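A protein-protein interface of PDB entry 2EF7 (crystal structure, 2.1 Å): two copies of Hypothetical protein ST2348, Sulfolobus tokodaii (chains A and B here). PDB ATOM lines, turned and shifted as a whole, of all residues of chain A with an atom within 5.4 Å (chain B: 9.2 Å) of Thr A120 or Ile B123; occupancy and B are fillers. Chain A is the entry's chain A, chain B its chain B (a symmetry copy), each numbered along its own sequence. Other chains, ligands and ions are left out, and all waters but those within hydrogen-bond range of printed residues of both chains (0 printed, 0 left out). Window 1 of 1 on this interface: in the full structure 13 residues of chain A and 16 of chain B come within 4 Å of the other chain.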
ATOM      1  N   LEU A  90       5.157  31.622  -5.415  1.00  0.00           N
ATOM      2  CA  LEU A  90       5.009  30.172  -5.423  1.00  0.00           C
ATOM      3  C   LEU A  90       3.571  29.756  -5.128  1.00  0.00           C
ATOM      4  O   LEU A  90       3.008  28.884  -5.794  1.00  0.00           O
ATOM      5  CB  LEU A  90       5.922  29.541  -4.378  1.00  0.00           C
ATOM      6  CG  LEU A  90       5.863  28.014  -4.325  1.00  0.00           C
ATOM      7  CD1 LEU A  90       6.238  27.423  -5.672  1.00  0.00           C
ATOM      8  CD2 LEU A  90       6.810  27.521  -3.245  1.00  0.00           C
ATOM      9  N   ILE A 116       8.909  29.344 -12.050  1.00  0.00           N
ATOM     10  CA  ILE A 116       9.088  28.356 -11.003  1.00  0.00           C
ATOM     11  C   ILE A 116      10.572  28.026 -10.817  1.00  0.00           C
ATOM     12  O   ILE A 116      11.007  27.717  -9.708  1.00  0.00           O
ATOM     13  CB  ILE A 116       8.302  27.064 -11.330  1.00  0.00           C
ATOM     14  CG1 ILE A 116       8.346  26.117 -10.131  1.00  0.00           C
ATOM     15  CG2 ILE A 116       8.861  26.410 -12.587  1.00  0.00           C
ATOM     16  CD1 ILE A 116       7.655  26.671  -8.903  1.00  0.00           C
ATOM     17  N   ARG A 117      11.350  28.096 -11.892  1.00  0.00           N
ATOM     18  CA  ARG A 117      12.779  27.813 -11.788  1.00  0.00           C
ATOM     19  C   ARG A 117      13.482  28.927 -11.032  1.00  0.00           C
ATOM     20  O   ARG A 117      14.484  28.686 -10.348  1.00  0.00           O
ATOM     21  CB  ARG A 117      13.421  27.654 -13.170  1.00  0.00           C
ATOM     22  CG  ARG A 117      12.921  26.462 -13.970  1.00  0.00           C
ATOM     23  CD  ARG A 117      12.910  25.183 -13.139  1.00  0.00           C
ATOM     24  NE  ARG A 117      12.583  24.011 -13.950  1.00  0.00           N
ATOM     25  CZ  ARG A 117      12.102  22.869 -13.466  1.00  0.00           C
ATOM     26  NH1 ARG A 117      11.879  22.735 -12.165  1.00  0.00           N
ATOM     27  NH2 ARG A 117      11.846  21.856 -14.285  1.00  0.00           N
ATOM     28  N   ASP A 118      12.970  30.152 -11.166  1.00  0.00           N
ATOM     29  CA  ASP A 118      13.560  31.285 -10.460  1.00  0.00           C
ATOM     30  C   ASP A 118      13.355  31.056  -8.964  1.00  0.00           C
ATOM     31  O   ASP A 118      14.212  31.396  -8.150  1.00  0.00           O
ATOM     32  CB  ASP A 118      12.892  32.603 -10.857  1.00  0.00           C
ATOM     33  CG  ASP A 118      13.235  33.036 -12.267  1.00  0.00           C
ATOM     34  OD1 ASP A 118      14.435  33.012 -12.626  1.00  0.00           O
ATOM     35  OD2 ASP A 118      12.306  33.416 -13.012  1.00  0.00           O
ATOM     36  N   ILE A 119      12.208  30.473  -8.617  1.00  0.00           N
ATOM     37  CA  ILE A 119      11.870  30.200  -7.225  1.00  0.00           C
ATOM     38  C   ILE A 119      12.799  29.175  -6.573  1.00  0.00           C
ATOM     39  O   ILE A 119      13.293  29.397  -5.470  1.00  0.00           O
ATOM     40  CB  ILE A 119      10.404  29.737  -7.103  1.00  0.00           C
ATOM     41  CG1 ILE A 119       9.481  30.872  -7.573  1.00  0.00           C
ATOM     42  CG2 ILE A 119      10.093  29.342  -5.659  1.00  0.00           C
ATOM     43  CD1 ILE A 119       8.009  30.569  -7.465  1.00  0.00           C
ATOM     44  N   THR A 120      13.044  28.061  -7.251  1.00  0.00           N
ATOM     45  CA  THR A 120      13.939  27.045  -6.695  1.00  0.00           C
ATOM     46  C   THR A 120      15.375  27.557  -6.619  1.00  0.00           C
ATOM     47  O   THR A 120      16.133  27.150  -5.739  1.00  0.00           O
ATOM     48  CB  THR A 120      13.911  25.748  -7.522  1.00  0.00           C
ATOM     49  OG1 THR A 120      14.106  26.056  -8.906  1.00  0.00           O
ATOM     50  CG2 THR A 120      12.587  25.033  -7.335  1.00  0.00           C
ATOM     51  N   ARG A 121      15.757  28.438  -7.539  1.00  0.00           N
ATOM     52  CA  ARG A 121      17.104  28.995  -7.509  1.00  0.00           C
ATOM     53  C   ARG A 121      17.230  29.876  -6.269  1.00  0.00           C
ATOM     54  O   ARG A 121      18.271  29.887  -5.608  1.00  0.00           O
ATOM     55  CB  ARG A 121      17.389  29.834  -8.763  1.00  0.00           C
ATOM     56  CG  ARG A 121      18.749  30.528  -8.723  1.00  0.00           C
ATOM     57  CD  ARG A 121      19.143  31.152 -10.063  1.00  0.00           C
ATOM     58  NE  ARG A 121      18.570  32.478 -10.295  1.00  0.00           N
ATOM     59  CZ  ARG A 121      17.410  32.706 -10.901  1.00  0.00           C
ATOM     60  NH1 ARG A 121      16.681  31.693 -11.345  1.00  0.00           N
ATOM     61  NH2 ARG A 121      16.982  33.952 -11.070  1.00  0.00           N
ATOM     62  N   ALA A 122      16.164  30.617  -5.969  1.00  0.00           N
ATOM     63  CA  ALA A 122      16.137  31.488  -4.800  1.00  0.00           C
ATOM     64  C   ALA A 122      16.220  30.644  -3.525  1.00  0.00           C
ATOM     65  O   ALA A 122      16.836  31.050  -2.534  1.00  0.00           O
ATOM     66  CB  ALA A 122      14.855  32.319  -4.795  1.00  0.00           C
ATOM     67  N   ILE A 123      15.598  29.470  -3.549  1.00  0.00           N
ATOM     68  CA  ILE A 123      15.637  28.597  -2.385  1.00  0.00           C
ATOM     69  C   ILE A 123      17.070  28.112  -2.225  1.00  0.00           C
ATOM     70  O   ILE A 123      17.650  28.202  -1.141  1.00  0.00           O
ATOM     71  CB  ILE A 123      14.691  27.387  -2.550  1.00  0.00           C
ATOM     72  CG1 ILE A 123      13.250  27.881  -2.688  1.00  0.00           C
ATOM     73  CG2 ILE A 123      14.811  26.454  -1.345  1.00  0.00           C
ATOM     74  CD1 ILE A 123      12.813  28.768  -1.555  1.00  0.00           C
ATOM     75  N   ASP A 124      17.647  27.615  -3.315  1.00  0.00           N
ATOM     76  CA  ASP A 124      19.026  27.142  -3.284  1.00  0.00           C
ATOM     77  C   ASP A 124      19.966  28.236  -2.803  1.00  0.00           C
ATOM     78  O   ASP A 124      20.865  27.989  -1.999  1.00  0.00           O
ATOM     79  CB  ASP A 124      19.459  26.676  -4.667  1.00  0.00           C
ATOM     80  CG  ASP A 124      19.043  25.256  -4.947  1.00  0.00           C
ATOM     81  OD1 ASP A 124      17.850  24.937  -4.760  1.00  0.00           O
ATOM     82  OD2 ASP A 124      19.913  24.457  -5.352  1.00  0.00           O
ATOM     83  N   ASP A 125      19.754  29.447  -3.297  1.00  0.00           N
ATOM     84  CA  ASP A 125      20.585  30.572  -2.910  1.00  0.00           C
ATOM     85  C   ASP A 125      20.613  30.815  -1.408  1.00  0.00           C
ATOM     86  O   ASP A 125      21.661  30.707  -0.783  1.00  0.00           O
ATOM     87  CB  ASP A 125      20.121  31.850  -3.611  1.00  0.00           C
ATOM     88  CG  ASP A 125      20.560  31.916  -5.062  1.00  0.00           C
ATOM     89  OD1 ASP A 125      20.343  32.977  -5.684  1.00  0.00           O
ATOM     90  OD2 ASP A 125      21.118  30.919  -5.578  1.00  0.00           O
ATOM     91  N   GLU B   4       0.644  19.058  -0.824  1.00  0.00           N
ATOM     92  CA  GLU B   4       1.729  18.096  -0.478  1.00  0.00           C
ATOM     93  C   GLU B   4       2.149  18.276   0.976  1.00  0.00           C
ATOM     94  O   GLU B   4       2.297  19.403   1.447  1.00  0.00           O
ATOM     95  CB  GLU B   4       2.925  18.312  -1.400  1.00  0.00           C
ATOM     96  CG  GLU B   4       2.532  18.461  -2.859  1.00  0.00           C
ATOM     97  CD  GLU B   4       3.670  18.154  -3.805  1.00  0.00           C
ATOM     98  OE1 GLU B   4       4.773  18.707  -3.607  1.00  0.00           O
ATOM     99  OE2 GLU B   4       3.462  17.362  -4.750  1.00  0.00           O
ATOM    100  N   TYR B   9       7.450  13.511   1.785  1.00  0.00           N
ATOM    101  CA  TYR B   9       8.765  13.875   1.269  1.00  0.00           C
ATOM    102  C   TYR B   9       9.918  13.696   2.243  1.00  0.00           C
ATOM    103  O   TYR B   9      11.083  13.677   1.843  1.00  0.00           O
ATOM    104  CB  TYR B   9       8.722  15.311   0.742  1.00  0.00           C
ATOM    105  CG  TYR B   9       8.025  15.412  -0.596  1.00  0.00           C
ATOM    106  CD1 TYR B   9       8.683  15.044  -1.771  1.00  0.00           C
ATOM    107  CD2 TYR B   9       6.692  15.810  -0.686  1.00  0.00           C
ATOM    108  CE1 TYR B   9       8.032  15.064  -3.003  1.00  0.00           C
ATOM    109  CE2 TYR B   9       6.028  15.832  -1.915  1.00  0.00           C
ATOM    110  CZ  TYR B   9       6.707  15.455  -3.068  1.00  0.00           C
ATOM    111  OH  TYR B   9       6.061  15.456  -4.287  1.00  0.00           O
ATOM    112  N   PRO B  85       1.856  21.011   5.584  1.00  0.00           N
ATOM    113  CA  PRO B  85       2.147  21.236   4.166  1.00  0.00           C
ATOM    114  C   PRO B  85       3.645  21.510   4.018  1.00  0.00           C
ATOM    115  O   PRO B  85       4.256  22.081   4.921  1.00  0.00           O
ATOM    116  CB  PRO B  85       1.289  22.454   3.835  1.00  0.00           C
ATOM    117  CG  PRO B  85       1.245  23.196   5.136  1.00  0.00           C
ATOM    118  CD  PRO B  85       1.023  22.095   6.133  1.00  0.00           C
ATOM    119  N   ILE B  86       4.246  21.106   2.902  1.00  0.00           N
ATOM    120  CA  ILE B  86       5.679  21.325   2.735  1.00  0.00           C
ATOM    121  C   ILE B  86       6.059  22.794   2.837  1.00  0.00           C
ATOM    122  O   ILE B  86       7.129  23.124   3.338  1.00  0.00           O
ATOM    123  CB  ILE B  86       6.212  20.789   1.391  1.00  0.00           C
ATOM    124  CG1 ILE B  86       5.406  21.378   0.242  1.00  0.00           C
ATOM    125  CG2 ILE B  86       6.181  19.264   1.382  1.00  0.00           C
ATOM    126  CD1 ILE B  86       5.939  20.993  -1.119  1.00  0.00           C
ATOM    127  N   THR B  87       5.189  23.676   2.366  1.00  0.00           N
ATOM    128  CA  THR B  87       5.486  25.098   2.428  1.00  0.00           C
ATOM    129  C   THR B  87       5.612  25.526   3.882  1.00  0.00           C
ATOM    130  O   THR B  87       6.228  26.539   4.181  1.00  0.00           O
ATOM    131  CB  THR B  87       4.395  25.935   1.732  1.00  0.00           C
ATOM    132  OG1 THR B  87       3.119  25.631   2.296  1.00  0.00           O
ATOM    133  CG2 THR B  87       4.376  25.635   0.241  1.00  0.00           C
ATOM    134  N   GLY B  88       5.017  24.747   4.782  1.00  0.00           N
ATOM    135  CA  GLY B  88       5.108  25.053   6.200  1.00  0.00           C
ATOM    136  C   GLY B  88       6.500  24.708   6.704  1.00  0.00           C
ATOM    137  O   GLY B  88       7.050  25.384   7.571  1.00  0.00           O
ATOM    138  N   LEU B  90       9.212  24.682   4.778  1.00  0.00           N
ATOM    139  CA  LEU B  90      10.099  25.666   4.168  1.00  0.00           C
ATOM    140  C   LEU B  90      10.178  26.940   5.001  1.00  0.00           C
ATOM    141  O   LEU B  90      11.266  27.481   5.209  1.00  0.00           O
ATOM    142  CB  LEU B  90       9.628  26.009   2.749  1.00  0.00           C
ATOM    143  CG  LEU B  90      10.486  27.041   2.006  1.00  0.00           C
ATOM    144  CD1 LEU B  90      11.932  26.561   1.924  1.00  0.00           C
ATOM    145  CD2 LEU B  90       9.915  27.270   0.619  1.00  0.00           C
ATOM    146  N   MET B  93      12.324  26.388   8.235  1.00  0.00           N
ATOM    147  CA  MET B  93      13.743  26.264   7.920  1.00  0.00           C
ATOM    148  C   MET B  93      14.345  27.627   7.663  1.00  0.00           C
ATOM    149  O   MET B  93      15.476  27.886   8.050  1.00  0.00           O
ATOM    150  CB  MET B  93      13.952  25.388   6.691  1.00  0.00           C
ATOM    151  CG  MET B  93      13.858  23.897   6.969  1.00  0.00           C
ATOM    152  SD  MET B  93      13.958  22.851   5.344  1.00  0.00           S
ATOM    153  CE  MET B  93      12.076  22.476   5.144  1.00  0.00           C
ATOM    154  N   SER B 115      14.559  17.672   4.733  1.00  0.00           N
ATOM    155  CA  SER B 115      15.554  18.696   4.425  1.00  0.00           C
ATOM    156  C   SER B 115      15.153  19.584   3.249  1.00  0.00           C
ATOM    157  O   SER B 115      14.202  19.292   2.525  1.00  0.00           O
ATOM    158  CB  SER B 115      16.885  18.027   4.099  1.00  0.00           C
ATOM    159  OG  SER B 115      16.788  17.343   2.860  1.00  0.00           O
ATOM    160  N   ILE B 116      15.895  20.671   3.061  1.00  0.00           N
ATOM    161  CA  ILE B 116      15.625  21.597   1.972  1.00  0.00           C
ATOM    162  C   ILE B 116      15.606  20.865   0.631  1.00  0.00           C
ATOM    163  O   ILE B 116      14.835  21.225  -0.261  1.00  0.00           O
ATOM    164  CB  ILE B 116      16.683  22.728   1.920  1.00  0.00           C
ATOM    165  CG1 ILE B 116      16.416  23.735   3.035  1.00  0.00           C
ATOM    166  CG2 ILE B 116      16.606  23.466   0.585  1.00  0.00           C
ATOM    167  CD1 ILE B 116      15.112  24.499   2.842  1.00  0.00           C
ATOM    168  N   ARG B 117      16.457  19.842   0.500  1.00  0.00           N
ATOM    169  CA  ARG B 117      16.546  19.051  -0.723  1.00  0.00           C
ATOM    170  C   ARG B 117      15.196  18.437  -1.034  1.00  0.00           C
ATOM    171  O   ARG B 117      14.755  18.416  -2.185  1.00  0.00           O
ATOM    172  CB  ARG B 117      17.584  17.939  -0.563  1.00  0.00           C
ATOM    173  CG  ARG B 117      19.021  18.424  -0.480  1.00  0.00           C
ATOM    174  CD  ARG B 117      19.673  18.460  -1.849  1.00  0.00           C
ATOM    175  NE  ARG B 117      18.926  19.280  -2.796  1.00  0.00           N
ATOM    176  CZ  ARG B 117      19.217  19.375  -4.091  1.00  0.00           C
ATOM    177  NH1 ARG B 117      20.240  18.696  -4.593  1.00  0.00           N
ATOM    178  NH2 ARG B 117      18.485  20.148  -4.882  1.00  0.00           N
ATOM    179  N   ASP B 118      14.550  17.925   0.007  1.00  0.00           N
ATOM    180  CA  ASP B 118      13.246  17.309  -0.131  1.00  0.00           C
ATOM    181  C   ASP B 118      12.246  18.366  -0.596  1.00  0.00           C
ATOM    182  O   ASP B 118      11.403  18.106  -1.456  1.00  0.00           O
ATOM    183  CB  ASP B 118      12.816  16.726   1.212  1.00  0.00           C
ATOM    184  CG  ASP B 118      13.762  15.655   1.709  1.00  0.00           C
ATOM    185  OD1 ASP B 118      13.928  15.539   2.939  1.00  0.00           O
ATOM    186  OD2 ASP B 118      14.331  14.920   0.874  1.00  0.00           O
ATOM    187  N   ILE B 119      12.352  19.560  -0.022  1.00  0.00           N
ATOM    188  CA  ILE B 119      11.458  20.651  -0.372  1.00  0.00           C
ATOM    189  C   ILE B 119      11.593  21.025  -1.849  1.00  0.00           C
ATOM    190  O   ILE B 119      10.599  21.038  -2.576  1.00  0.00           O
ATOM    191  CB  ILE B 119      11.743  21.901   0.480  1.00  0.00           C
ATOM    192  CG1 ILE B 119      11.645  21.558   1.967  1.00  0.00           C
ATOM    193  CG2 ILE B 119      10.750  23.007   0.133  1.00  0.00           C
ATOM    194  CD1 ILE B 119      10.249  21.236   2.428  1.00  0.00           C
ATOM    195  N   THR B 120      12.811  21.331  -2.299  1.00  0.00           N
ATOM    196  CA  THR B 120      12.994  21.703  -3.702  1.00  0.00           C
ATOM    197  C   THR B 120      12.578  20.541  -4.593  1.00  0.00           C
ATOM    198  O   THR B 120      12.078  20.749  -5.698  1.00  0.00           O
ATOM    199  CB  THR B 120      14.459  22.116  -4.022  1.00  0.00           C
ATOM    200  OG1 THR B 120      15.359  21.060  -3.673  1.00  0.00           O
ATOM    201  CG2 THR B 120      14.831  23.365  -3.249  1.00  0.00           C
ATOM    202  N   ARG B 121      12.767  19.316  -4.103  1.00  0.00           N
ATOM    203  CA  ARG B 121      12.370  18.139  -4.864  1.00  0.00           C
ATOM    204  C   ARG B 121      10.853  18.179  -5.055  1.00  0.00           C
ATOM    205  O   ARG B 121      10.354  18.138  -6.183  1.00  0.00           O
ATOM    206  CB  ARG B 121      12.773  16.855  -4.127  1.00  0.00           C
ATOM    207  CG  ARG B 121      12.307  15.568  -4.813  1.00  0.00           C
ATOM    208  CD  ARG B 121      13.154  14.357  -4.404  1.00  0.00           C
ATOM    209  NE  ARG B 121      13.037  14.005  -2.987  1.00  0.00           N
ATOM    210  CZ  ARG B 121      11.975  13.419  -2.441  1.00  0.00           C
ATOM    211  NH1 ARG B 121      10.923  13.114  -3.189  1.00  0.00           N
ATOM    212  NH2 ARG B 121      11.965  13.134  -1.143  1.00  0.00           N
ATOM    213  N   ALA B 122      10.123  18.271  -3.949  1.00  0.00           N
ATOM    214  CA  ALA B 122       8.669  18.318  -4.015  1.00  0.00           C
ATOM    215  C   ALA B 122       8.242  19.404  -4.994  1.00  0.00           C
ATOM    216  O   ALA B 122       7.272  19.231  -5.734  1.00  0.00           O
ATOM    217  CB  ALA B 122       8.086  18.594  -2.634  1.00  0.00           C
ATOM    218  N   ILE B 123       8.963  20.524  -5.002  1.00  0.00           N
ATOM    219  CA  ILE B 123       8.626  21.602  -5.917  1.00  0.00           C
ATOM    220  C   ILE B 123       8.830  21.121  -7.347  1.00  0.00           C
ATOM    221  O   ILE B 123       7.965  21.314  -8.195  1.00  0.00           O
ATOM    222  CB  ILE B 123       9.473  22.877  -5.648  1.00  0.00           C
ATOM    223  CG1 ILE B 123       8.839  23.706  -4.529  1.00  0.00           C
ATOM    224  CG2 ILE B 123       9.535  23.748  -6.894  1.00  0.00           C
ATOM    225  CD1 ILE B 123       8.594  22.951  -3.256  1.00  0.00           C
ATOM    226  N   ASP B 124       9.959  20.475  -7.619  1.00  0.00           N
ATOM    227  CA  ASP B 124      10.214  19.980  -8.967  1.00  0.00           C
ATOM    228  C   ASP B 124       9.086  19.081  -9.454  1.00  0.00           C
ATOM    229  O   ASP B 124       8.676  19.173 -10.607  1.00  0.00           O
ATOM    230  CB  ASP B 124      11.526  19.203  -9.029  1.00  0.00           C
ATOM    231  CG  ASP B 124      12.738  20.087  -8.855  1.00  0.00           C
ATOM    232  OD1 ASP B 124      12.696  21.250  -9.317  1.00  0.00           O
ATOM    233  OD2 ASP B 124      13.738  19.612  -8.271  1.00  0.00           O
ATOM    234  N   ASP B 125       8.579  18.219  -8.572  1.00  0.00           N
ATOM    235  CA  ASP B 125       7.499  17.299  -8.934  1.00  0.00           C
ATOM    236  C   ASP B 125       6.167  17.960  -9.277  1.00  0.00           C
ATOM    237  O   ASP B 125       5.263  17.302  -9.784  1.00  0.00           O
ATOM    238  CB  ASP B 125       7.272  16.279  -7.816  1.00  0.00           C
ATOM    239  CG  ASP B 125       8.446  15.345  -7.639  1.00  0.00           C
ATOM    240  OD1 ASP B 125       9.094  15.014  -8.654  1.00  0.00           O
ATOM    241  OD2 ASP B 125       8.717  14.933  -6.492  1.00  0.00           O
ATOM    242  N   MET B 126       6.044  19.253  -9.001  1.00  0.00           N
ATOM    243  CA  MET B 126       4.808  19.972  -9.288  1.00  0.00           C
ATOM    244  C   MET B 126       5.013  21.016 -10.381  1.00  0.00           C
ATOM    245  O   MET B 126       5.451  20.697 -11.490  1.00  0.00           O
ATOM    246  CB  MET B 126       4.289  20.644  -8.013  1.00  0.00           C
ATOM    247  CG  MET B 126       5.293  21.590  -7.363  1.00  0.00           C
ATOM    248  SD  MET B 126       4.649  22.499  -5.774  1.00  0.00           S
ATOM    249  CE  MET B 126       5.451  21.390  -4.417  1.00  0.00           C
ATOM    250  N   MET B 130       2.245  21.526 -14.492  1.00  0.00           N
ATOM    251  CA  MET B 130       1.795  22.915 -14.593  1.00  0.00           C
ATOM    252  C   MET B 130       1.803  23.389 -16.043  1.00  0.00           C
ATOM    253  O   MET B 130       2.593  22.906 -16.858  1.00  0.00           O
ATOM    254  CB  MET B 130       2.709  23.840 -13.780  1.00  0.00           C
ATOM    255  CG  MET B 130       2.826  23.499 -12.298  1.00  0.00           C
ATOM    256  SD  MET B 130       4.259  24.488 -11.400  1.00  0.00           S
ATOM    257  CE  MET B 130       3.214  25.545 -10.138  1.00  0.00           C
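OD1 of Asp B124 lies within salt-bridge range of NH1 of Arg A117.
Arg A117 touches Asp B124, but with the chains exchanged Asp A124 does not touch Arg B117 (4.6 Å). Thr A120 touches Ile B123, and with the chains exchanged Ile A123 touches Thr B120. Ile A123 touches Leu B90, but with the chains exchanged Leu A90 does not touch Ile B123 (4.5 Å). Ile A123 touches Ile B116, but with the chains exchanged Ile A116 does not touch Ile B123 (4.01 Å). 11 positions are printed for both chains. Of the 6 pairs that touch across the chains among the printed residues, 2 have their exchanged pair printed and touching as well.
Of the 11 printed residues of chain A, 4 touch a printed residue of chain B. Printed residues of chain B that touch a printed residue of chain A: Leu B90, Ile B116, Thr B120, Ile B123 and Asp B124. Among the printed residues, Asp or Glu carboxylates within 4 Å of a Lys or Arg side-chain nitrogen of the other chain: Arg A117 with Asp B124.
Thr A120 touches just one residue of chain B: Ile B123 (3.3 Å). Of the printed residues of chain A, Ile B123 touches Thr A120 (3.3 Å). No residue of chain B comes within 4 Å of Ala A122. Printed residues of chain B within 4 Å of Asp A124: Thr B120 (3.7 Å). Printed residues of chain A within 4 Å of Thr B120: Ile A123 (3.6 Å) and Asp A124 (3.7 Å). The nearest residue of chain B that does not touch Thr A120 is Asp B124 (4.3 Å). The nearest printed residue of chain A that does not touch Ile B123 is Ile A116 (4.01 Å). The nearest printed residue of chain B that does not touch Asp A124 is Arg B117 (4.6 Å).
Ile B123 touches Thr A120 (CG2 to CG2, 3.3 Å). Leu B90 touches Ile A123 (CD2 to CD1, 3.9 Å). CG2 of Ile A123 touches CG2 of Ile B116 (3.98 Å). CG2 of Thr B120 touches CG2 of Ile A123, 3.6 Å away. Asp A124 touches Thr B120 (OD1 to CG2, 3.7 Å).
The backbone carbonyl oxygen (O) of Arg A117 lies within hydrogen-bond range of the side-chain hydroxyl (OG1) of Thr A120. O of Ile B116 lies within hydrogen-bond range of OG1 of Thr B120, at 3.5 Å. The backbone NH (N) of Ile B116 lies close to the side-chain sulfur (SD) of Met B93, at 3.7 Å. The backbone carbonyl oxygen (O) of Arg B117 is in hydrogen-bond range of the side-chain hydroxyl (OG1) of Thr B120, 3.1 Å away.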
